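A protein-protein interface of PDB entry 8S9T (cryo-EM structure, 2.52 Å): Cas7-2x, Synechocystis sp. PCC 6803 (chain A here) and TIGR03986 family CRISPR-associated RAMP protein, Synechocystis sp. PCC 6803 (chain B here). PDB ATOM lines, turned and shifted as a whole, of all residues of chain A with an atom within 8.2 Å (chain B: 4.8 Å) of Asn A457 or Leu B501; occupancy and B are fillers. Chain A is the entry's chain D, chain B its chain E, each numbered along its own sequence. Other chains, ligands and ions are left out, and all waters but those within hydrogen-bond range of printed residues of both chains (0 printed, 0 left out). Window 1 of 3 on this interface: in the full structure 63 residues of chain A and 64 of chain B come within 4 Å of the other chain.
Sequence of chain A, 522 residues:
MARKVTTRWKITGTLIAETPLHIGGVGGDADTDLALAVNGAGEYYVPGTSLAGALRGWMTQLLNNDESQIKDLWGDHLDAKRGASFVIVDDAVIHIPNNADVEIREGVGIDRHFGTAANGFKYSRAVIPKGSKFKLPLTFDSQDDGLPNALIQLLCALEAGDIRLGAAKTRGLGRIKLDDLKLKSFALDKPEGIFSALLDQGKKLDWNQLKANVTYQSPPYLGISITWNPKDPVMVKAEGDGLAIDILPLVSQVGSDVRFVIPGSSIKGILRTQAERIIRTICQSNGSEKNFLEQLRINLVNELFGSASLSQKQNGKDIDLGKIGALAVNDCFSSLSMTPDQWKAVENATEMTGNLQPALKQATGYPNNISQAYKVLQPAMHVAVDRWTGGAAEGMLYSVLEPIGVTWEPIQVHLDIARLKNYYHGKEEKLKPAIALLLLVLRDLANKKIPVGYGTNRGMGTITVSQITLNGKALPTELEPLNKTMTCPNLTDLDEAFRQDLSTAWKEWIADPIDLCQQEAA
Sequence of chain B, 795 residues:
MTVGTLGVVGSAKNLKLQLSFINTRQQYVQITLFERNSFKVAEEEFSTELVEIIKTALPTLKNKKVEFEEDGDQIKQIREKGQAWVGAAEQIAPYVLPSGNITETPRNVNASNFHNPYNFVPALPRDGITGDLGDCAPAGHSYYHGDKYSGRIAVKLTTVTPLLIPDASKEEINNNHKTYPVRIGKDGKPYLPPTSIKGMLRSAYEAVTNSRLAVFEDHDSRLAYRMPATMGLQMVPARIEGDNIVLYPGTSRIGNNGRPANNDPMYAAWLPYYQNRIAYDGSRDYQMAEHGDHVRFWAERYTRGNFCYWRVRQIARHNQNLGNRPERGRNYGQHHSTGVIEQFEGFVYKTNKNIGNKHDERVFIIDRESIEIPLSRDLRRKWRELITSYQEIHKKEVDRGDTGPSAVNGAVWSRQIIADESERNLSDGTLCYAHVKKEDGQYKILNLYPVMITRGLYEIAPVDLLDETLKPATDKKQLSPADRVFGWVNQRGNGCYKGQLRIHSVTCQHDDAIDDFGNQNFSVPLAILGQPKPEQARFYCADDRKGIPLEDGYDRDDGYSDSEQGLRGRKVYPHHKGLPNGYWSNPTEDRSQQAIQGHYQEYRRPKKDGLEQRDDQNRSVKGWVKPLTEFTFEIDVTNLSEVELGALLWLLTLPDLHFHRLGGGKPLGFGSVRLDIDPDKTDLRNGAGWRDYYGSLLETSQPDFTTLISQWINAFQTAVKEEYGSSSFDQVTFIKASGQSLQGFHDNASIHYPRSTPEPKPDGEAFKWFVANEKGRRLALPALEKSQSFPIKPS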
ATOM      1  N   PHE A 114      12.086 -34.387  16.238  1.00  0.00           N
ATOM      2  CA  PHE A 114      11.052 -33.457  16.670  1.00  0.00           C
ATOM      3  C   PHE A 114      11.495 -32.008  16.687  1.00  0.00           C
ATOM      4  O   PHE A 114      10.638 -31.126  16.665  1.00  0.00           O
ATOM      5  CB  PHE A 114      10.529 -33.847  18.046  1.00  0.00           C
ATOM      6  CG  PHE A 114       9.827 -35.154  18.066  1.00  0.00           C
ATOM      7  CD1 PHE A 114       8.590 -35.280  17.468  1.00  0.00           C
ATOM      8  CD2 PHE A 114      10.397 -36.262  18.649  1.00  0.00           C
ATOM      9  CE1 PHE A 114       7.938 -36.469  17.472  1.00  0.00           C
ATOM     10  CE2 PHE A 114       9.747 -37.457  18.648  1.00  0.00           C
ATOM     11  CZ  PHE A 114       8.517 -37.563  18.062  1.00  0.00           C
ATOM     12  N   GLY A 115      12.793 -31.736  16.715  1.00  0.00           N
ATOM     13  CA  GLY A 115      13.260 -30.374  16.737  1.00  0.00           C
ATOM     14  C   GLY A 115      13.142 -29.706  18.076  1.00  0.00           C
ATOM     15  O   GLY A 115      13.098 -28.476  18.147  1.00  0.00           O
ATOM     16  N   PRO A 451      18.669 -20.797  11.197  1.00  0.00           N
ATOM     17  CA  PRO A 451      18.401 -19.805  12.236  1.00  0.00           C
ATOM     18  C   PRO A 451      19.098 -20.161  13.540  1.00  0.00           C
ATOM     19  O   PRO A 451      19.394 -21.322  13.819  1.00  0.00           O
ATOM     20  CB  PRO A 451      16.878 -19.858  12.369  1.00  0.00           C
ATOM     21  CG  PRO A 451      16.554 -21.226  12.015  1.00  0.00           C
ATOM     22  CD  PRO A 451      17.498 -21.648  10.952  1.00  0.00           C
ATOM     23  N   GLY A 453      19.530 -19.616  17.840  1.00  0.00           N
ATOM     24  CA  GLY A 453      18.987 -19.260  19.128  1.00  0.00           C
ATOM     25  C   GLY A 453      17.516 -19.568  19.339  1.00  0.00           C
ATOM     26  O   GLY A 453      16.920 -20.465  18.744  1.00  0.00           O
ATOM     27  N   TYR A 454      16.941 -18.799  20.250  1.00  0.00           N
ATOM     28  CA  TYR A 454      15.573 -18.978  20.701  1.00  0.00           C
ATOM     29  C   TYR A 454      14.567 -18.539  19.652  1.00  0.00           C
ATOM     30  O   TYR A 454      14.832 -17.648  18.848  1.00  0.00           O
ATOM     31  CB  TYR A 454      15.366 -18.167  21.981  1.00  0.00           C
ATOM     32  CG  TYR A 454      14.101 -18.461  22.720  1.00  0.00           C
ATOM     33  CD1 TYR A 454      13.903 -19.680  23.336  1.00  0.00           C
ATOM     34  CD2 TYR A 454      13.099 -17.510  22.804  1.00  0.00           C
ATOM     35  CE1 TYR A 454      12.750 -19.951  23.989  1.00  0.00           C
ATOM     36  CE2 TYR A 454      11.948 -17.771  23.454  1.00  0.00           C
ATOM     37  CZ  TYR A 454      11.778 -18.988  24.061  1.00  0.00           C
ATOM     38  OH  TYR A 454      10.614 -19.258  24.740  1.00  0.00           O
ATOM     39  N   GLY A 455      13.396 -19.168  19.679  1.00  0.00           N
ATOM     40  CA  GLY A 455      12.232 -18.615  19.014  1.00  0.00           C
ATOM     41  C   GLY A 455      12.345 -18.510  17.512  1.00  0.00           C
ATOM     42  O   GLY A 455      11.899 -17.516  16.937  1.00  0.00           O
ATOM     43  N   THR A 456      12.961 -19.491  16.866  1.00  0.00           N
ATOM     44  CA  THR A 456      13.248 -19.380  15.440  1.00  0.00           C
ATOM     45  C   THR A 456      11.995 -19.482  14.576  1.00  0.00           C
ATOM     46  O   THR A 456      11.905 -18.817  13.542  1.00  0.00           O
ATOM     47  CB  THR A 456      14.289 -20.411  15.034  1.00  0.00           C
ATOM     48  OG1 THR A 456      13.806 -21.720  15.320  1.00  0.00           O
ATOM     49  CG2 THR A 456      15.582 -20.169  15.785  1.00  0.00           C
ATOM     50  N   ASN A 457      11.019 -20.293  14.966  1.00  0.00           N
ATOM     51  CA  ASN A 457       9.722 -20.297  14.305  1.00  0.00           C
ATOM     52  C   ASN A 457       8.783 -19.241  14.838  1.00  0.00           C
ATOM     53  O   ASN A 457       7.640 -19.181  14.399  1.00  0.00           O
ATOM     54  CB  ASN A 457       9.047 -21.651  14.460  1.00  0.00           C
ATOM     55  CG  ASN A 457       9.699 -22.716  13.670  1.00  0.00           C
ATOM     56  OD1 ASN A 457      10.427 -22.450  12.739  1.00  0.00           O
ATOM     57  ND2 ASN A 457       9.487 -23.939  14.067  1.00  0.00           N
ATOM     58  N   ARG A 458       9.236 -18.406  15.756  1.00  0.00           N
ATOM     59  CA  ARG A 458       8.418 -17.452  16.480  1.00  0.00           C
ATOM     60  C   ARG A 458       9.033 -16.070  16.383  1.00  0.00           C
ATOM     61  O   ARG A 458       9.048 -15.297  17.339  1.00  0.00           O
ATOM     62  CB  ARG A 458       8.186 -17.899  17.924  1.00  0.00           C
ATOM     63  CG  ARG A 458       7.710 -19.332  17.998  1.00  0.00           C
ATOM     64  CD  ARG A 458       7.109 -19.791  19.316  1.00  0.00           C
ATOM     65  NE  ARG A 458       7.913 -19.601  20.519  1.00  0.00           N
ATOM     66  CZ  ARG A 458       9.085 -20.173  20.748  1.00  0.00           C
ATOM     67  NH1 ARG A 458       9.571 -21.059  19.910  1.00  0.00           N
ATOM     68  NH2 ARG A 458       9.723 -19.934  21.869  1.00  0.00           N
ATOM     69  N   GLY A 459       9.537 -15.748  15.197  1.00  0.00           N
ATOM     70  CA  GLY A 459       9.901 -14.406  14.812  1.00  0.00           C
ATOM     71  C   GLY A 459      11.309 -13.980  15.136  1.00  0.00           C
ATOM     72  O   GLY A 459      11.621 -12.793  15.015  1.00  0.00           O
ATOM     73  N   MET A 460      12.170 -14.900  15.532  1.00  0.00           N
ATOM     74  CA  MET A 460      13.540 -14.571  15.860  1.00  0.00           C
ATOM     75  C   MET A 460      14.489 -15.488  15.100  1.00  0.00           C
ATOM     76  O   MET A 460      14.079 -16.482  14.511  1.00  0.00           O
ATOM     77  CB  MET A 460      13.745 -14.678  17.368  1.00  0.00           C
ATOM     78  CG  MET A 460      13.020 -13.606  18.153  1.00  0.00           C
ATOM     79  SD  MET A 460      13.810 -13.212  19.711  1.00  0.00           S
ATOM     80  CE  MET A 460      13.534 -14.736  20.590  1.00  0.00           C
ATOM     81  N   GLY A 461      15.766 -15.132  15.091  1.00  0.00           N
ATOM     82  CA  GLY A 461      16.828 -16.060  14.764  1.00  0.00           C
ATOM     83  C   GLY A 461      17.353 -16.088  13.343  1.00  0.00           C
ATOM     84  O   GLY A 461      18.391 -16.709  13.124  1.00  0.00           O
ATOM     85  N   THR A 462      16.695 -15.468  12.371  1.00  0.00           N
ATOM     86  CA  THR A 462      17.282 -15.401  11.039  1.00  0.00           C
ATOM     87  C   THR A 462      18.401 -14.371  10.992  1.00  0.00           C
ATOM     88  O   THR A 462      18.299 -13.290  11.566  1.00  0.00           O
ATOM     89  CB  THR A 462      16.224 -15.111   9.967  1.00  0.00           C
ATOM     90  OG1 THR A 462      16.830 -15.118   8.672  1.00  0.00           O
ATOM     91  CG2 THR A 462      15.593 -13.808  10.168  1.00  0.00           C
ATOM     92  N   LYS B 198       2.298 -15.075  11.702  1.00  0.00           N
ATOM     93  CA  LYS B 198       2.161 -16.498  11.970  1.00  0.00           C
ATOM     94  C   LYS B 198       0.788 -16.839  12.527  1.00  0.00           C
ATOM     95  O   LYS B 198       0.178 -17.828  12.114  1.00  0.00           O
ATOM     96  CB  LYS B 198       3.258 -16.958  12.923  1.00  0.00           C
ATOM     97  CG  LYS B 198       3.374 -18.446  13.045  1.00  0.00           C
ATOM     98  CD  LYS B 198       4.434 -18.846  14.024  1.00  0.00           C
ATOM     99  CE  LYS B 198       4.635 -20.331  14.021  1.00  0.00           C
ATOM    100  NZ  LYS B 198       5.586 -20.776  15.053  1.00  0.00           N
ATOM    101  N   VAL B 485       2.220 -28.548  10.745  1.00  0.00           N
ATOM    102  CA  VAL B 485       2.790 -27.432  10.001  1.00  0.00           C
ATOM    103  C   VAL B 485       3.335 -26.371  10.943  1.00  0.00           C
ATOM    104  O   VAL B 485       4.454 -25.890  10.770  1.00  0.00           O
ATOM    105  CB  VAL B 485       1.751 -26.853   9.027  1.00  0.00           C
ATOM    106  CG1 VAL B 485       2.304 -25.648   8.329  1.00  0.00           C
ATOM    107  CG2 VAL B 485       1.376 -27.888   8.012  1.00  0.00           C
ATOM    108  N   PHE B 486       2.549 -25.960  11.926  1.00  0.00           N
ATOM    109  CA  PHE B 486       2.943 -24.863  12.796  1.00  0.00           C
ATOM    110  C   PHE B 486       3.531 -25.295  14.127  1.00  0.00           C
ATOM    111  O   PHE B 486       3.954 -24.433  14.894  1.00  0.00           O
ATOM    112  CB  PHE B 486       1.767 -23.930  13.031  1.00  0.00           C
ATOM    113  CG  PHE B 486       1.322 -23.234  11.803  1.00  0.00           C
ATOM    114  CD1 PHE B 486       0.438 -23.831  10.932  1.00  0.00           C
ATOM    115  CD2 PHE B 486       1.816 -21.988  11.492  1.00  0.00           C
ATOM    116  CE1 PHE B 486       0.047 -23.192   9.799  1.00  0.00           C
ATOM    117  CE2 PHE B 486       1.418 -21.353  10.357  1.00  0.00           C
ATOM    118  CZ  PHE B 486       0.536 -21.955   9.513  1.00  0.00           C
ATOM    119  N   LYS B 498       8.448 -29.118  17.022  1.00  0.00           N
ATOM    120  CA  LYS B 498       8.863 -27.905  16.345  1.00  0.00           C
ATOM    121  C   LYS B 498       8.073 -27.724  15.056  1.00  0.00           C
ATOM    122  O   LYS B 498       7.863 -28.667  14.301  1.00  0.00           O
ATOM    123  CB  LYS B 498      10.355 -27.944  16.068  1.00  0.00           C
ATOM    124  CG  LYS B 498      10.874 -26.685  15.472  1.00  0.00           C
ATOM    125  CD  LYS B 498      12.340 -26.748  15.315  1.00  0.00           C
ATOM    126  CE  LYS B 498      12.863 -25.453  14.799  1.00  0.00           C
ATOM    127  NZ  LYS B 498      14.331 -25.467  14.718  1.00  0.00           N
ATOM    128  N   GLY B 499       7.644 -26.493  14.810  1.00  0.00           N
ATOM    129  CA  GLY B 499       6.911 -26.202  13.594  1.00  0.00           C
ATOM    130  C   GLY B 499       7.730 -26.453  12.345  1.00  0.00           C
ATOM    131  O   GLY B 499       8.932 -26.192  12.296  1.00  0.00           O
ATOM    132  N   GLN B 500       7.074 -27.014  11.344  1.00  0.00           N
ATOM    133  CA  GLN B 500       7.625 -27.183  10.011  1.00  0.00           C
ATOM    134  C   GLN B 500       7.539 -25.932   9.150  1.00  0.00           C
ATOM    135  O   GLN B 500       7.887 -25.998   7.977  1.00  0.00           O
ATOM    136  CB  GLN B 500       6.927 -28.344   9.322  1.00  0.00           C
ATOM    137  CG  GLN B 500       7.379 -29.672   9.830  1.00  0.00           C
ATOM    138  CD  GLN B 500       6.596 -30.803   9.246  1.00  0.00           C
ATOM    139  OE1 GLN B 500       6.064 -31.639   9.959  1.00  0.00           O
ATOM    140  NE2 GLN B 500       6.505 -30.831   7.937  1.00  0.00           N
ATOM    141  N   LEU B 501       7.041 -24.818   9.675  1.00  0.00           N
ATOM    142  CA  LEU B 501       6.863 -23.582   8.926  1.00  0.00           C
ATOM    143  C   LEU B 501       7.489 -22.442   9.705  1.00  0.00           C
ATOM    144  O   LEU B 501       7.235 -22.299  10.901  1.00  0.00           O
ATOM    145  CB  LEU B 501       5.378 -23.317   8.676  1.00  0.00           C
ATOM    146  CG  LEU B 501       4.875 -22.132   7.862  1.00  0.00           C
ATOM    147  CD1 LEU B 501       3.569 -22.477   7.228  1.00  0.00           C
ATOM    148  CD2 LEU B 501       4.689 -20.905   8.731  1.00  0.00           C
ATOM    149  N   ARG B 502       8.283 -21.621   9.027  1.00  0.00           N
ATOM    150  CA  ARG B 502       9.002 -20.516   9.648  1.00  0.00           C
ATOM    151  C   ARG B 502       8.770 -19.241   8.853  1.00  0.00           C
ATOM    152  O   ARG B 502       9.080 -19.187   7.664  1.00  0.00           O
ATOM    153  CB  ARG B 502      10.496 -20.834   9.739  1.00  0.00           C
ATOM    154  CG  ARG B 502      11.378 -19.689  10.127  1.00  0.00           C
ATOM    155  CD  ARG B 502      12.806 -20.150  10.275  1.00  0.00           C
ATOM    156  NE  ARG B 502      13.773 -19.079  10.049  1.00  0.00           N
ATOM    157  CZ  ARG B 502      14.703 -19.100   9.095  1.00  0.00           C
ATOM    158  NH1 ARG B 502      14.781 -20.115   8.243  1.00  0.00           N
ATOM    159  NH2 ARG B 502      15.547 -18.097   8.971  1.00  0.00           N
ATOM    160  N   ILE B 503       8.226 -18.225   9.500  1.00  0.00           N
ATOM    161  CA  ILE B 503       8.066 -16.900   8.911  1.00  0.00           C
ATOM    162  C   ILE B 503       9.231 -16.038   9.358  1.00  0.00           C
ATOM    163  O   ILE B 503       9.606 -16.050  10.532  1.00  0.00           O
ATOM    164  CB  ILE B 503       6.716 -16.273   9.298  1.00  0.00           C
ATOM    165  CG1 ILE B 503       5.589 -16.975   8.550  1.00  0.00           C
ATOM    166  CG2 ILE B 503       6.692 -14.796   9.018  1.00  0.00           C
ATOM    167  CD1 ILE B 503       4.321 -16.999   9.274  1.00  0.00           C
ATOM    168  N   ILE B 635       8.433 -17.432   3.920  1.00  0.00           N
ATOM    169  CA  ILE B 635       8.095 -18.631   4.669  1.00  0.00           C
ATOM    170  C   ILE B 635       9.098 -19.707   4.302  1.00  0.00           C
ATOM    171  O   ILE B 635       9.271 -20.030   3.124  1.00  0.00           O
ATOM    172  CB  ILE B 635       6.662 -19.096   4.384  1.00  0.00           C
ATOM    173  CG1 ILE B 635       5.697 -17.933   4.522  1.00  0.00           C
ATOM    174  CG2 ILE B 635       6.280 -20.211   5.303  1.00  0.00           C
ATOM    175  CD1 ILE B 635       4.278 -18.313   4.291  1.00  0.00           C
ATOM    176  N   ASP B 636       9.763 -20.255   5.299  1.00  0.00           N
ATOM    177  CA  ASP B 636      10.554 -21.459   5.131  1.00  0.00           C
ATOM    178  C   ASP B 636       9.735 -22.637   5.634  1.00  0.00           C
ATOM    179  O   ASP B 636       9.222 -22.599   6.753  1.00  0.00           O
ATOM    180  CB  ASP B 636      11.871 -21.318   5.889  1.00  0.00           C
ATOM    181  CG  ASP B 636      12.614 -22.620   6.034  1.00  0.00           C
ATOM    182  OD1 ASP B 636      12.705 -23.384   5.047  1.00  0.00           O
ATOM    183  OD2 ASP B 636      13.108 -22.886   7.150  1.00  0.00           O
ATOM    184  N   VAL B 637       9.589 -23.664   4.805  1.00  0.00           N
ATOM    185  CA  VAL B 637       8.794 -24.835   5.146  1.00  0.00           C
ATOM    186  C   VAL B 637       9.645 -26.083   4.981  1.00  0.00           C
ATOM    187  O   VAL B 637      10.539 -26.140   4.138  1.00  0.00           O
ATOM    188  CB  VAL B 637       7.496 -24.949   4.315  1.00  0.00           C
ATOM    189  CG1 VAL B 637       6.686 -23.687   4.427  1.00  0.00           C
ATOM    190  CG2 VAL B 637       7.787 -25.294   2.867  1.00  0.00           C
ATOM    191  N   LEU B 648      -1.518 -24.432   2.270  1.00  0.00           N
ATOM    192  CA  LEU B 648      -0.760 -23.204   2.455  1.00  0.00           C
ATOM    193  C   LEU B 648      -0.736 -22.363   1.187  1.00  0.00           C
ATOM    194  O   LEU B 648      -1.032 -21.165   1.224  1.00  0.00           O
ATOM    195  CB  LEU B 648       0.652 -23.545   2.926  1.00  0.00           C
ATOM    196  CG  LEU B 648       1.628 -22.390   3.108  1.00  0.00           C
ATOM    197  CD1 LEU B 648       1.138 -21.446   4.164  1.00  0.00           C
ATOM    198  CD2 LEU B 648       2.980 -22.919   3.482  1.00  0.00           C
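OG1 of Thr A462 lies close to NH2 of Arg B502 (3.3 Å).
O of Phe A114 sits at hydrogen-bond distance from N of Lys B498, at 3.0 Å.
NZ of Lys B198 lies within hydrogen-bond range of O of Asn A457 (2.7 Å).
The backbone carbonyl oxygen (O) of Gly B499 is in hydrogen-bond range of the side-chain amide nitrogen (ND2) of Asn A457 (2.9 Å).
The guanidinium group of Arg B502 lies within salt-bridge range of the side-chain carboxylate of Asp B636, 3.4 Å away.
OH of Tyr A454 is in hydrogen-bond range of NH2 of Arg A458.
The backbone carbonyl oxygen of Val B485 lies within hydrogen-bond range of the backbone NH of Leu B501 (3.0 Å).
O of Gly A115 touches CD of Lys B498, at 3.4 Å.
Pro A451 touches Arg B502 (CB to NE, 3.95 Å).
Lys B498 touches Thr A456 (NZ to OG1, 3.8 Å).
O of Thr A456 touches CG of Arg B502 (3.6 Å).
CG of Lys B498 touches ND2 of Asn A457 (3.4 Å).
OD1 of Asn A457 touches O of Leu B501, 3.7 Å away.
Asn A457 touches Arg B502.
NZ of Lys B198 touches CG of Arg A458, at 3.9 Å.
Of the printed residues of chain B, Thr A456 touches Lys B498 (3.8 Å) and Arg B502 (3.6 Å).
Of the printed residues of chain A, Lys B198 touches Asn A457 and Arg A458.
Of the printed residues of chain A, Gly B499 touches Asn A457.
Leu B501 touches just one residue of chain A: Asn A457.
The nearest printed residue of chain B that does not touch Asn A457 is Gln B500 (4.8 Å).
The nearest residue of chain A that does not touch Leu B501 is Thr A456 (6.4 Å).
The nearest printed residue of chain A that does not touch Arg B502 is Gly A461 (5.1 Å).
Hydrophobic or aromatic side chains of chain A that line the printed part of chain B: Pro A451.
Along chain B the printed residues that touch a printed residue of chain A span positions 198 to 502.
Among the printed residues, no Asp or Glu carboxylate lies within 4 Å of a Lys or Arg side-chain nitrogen of the other chain.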
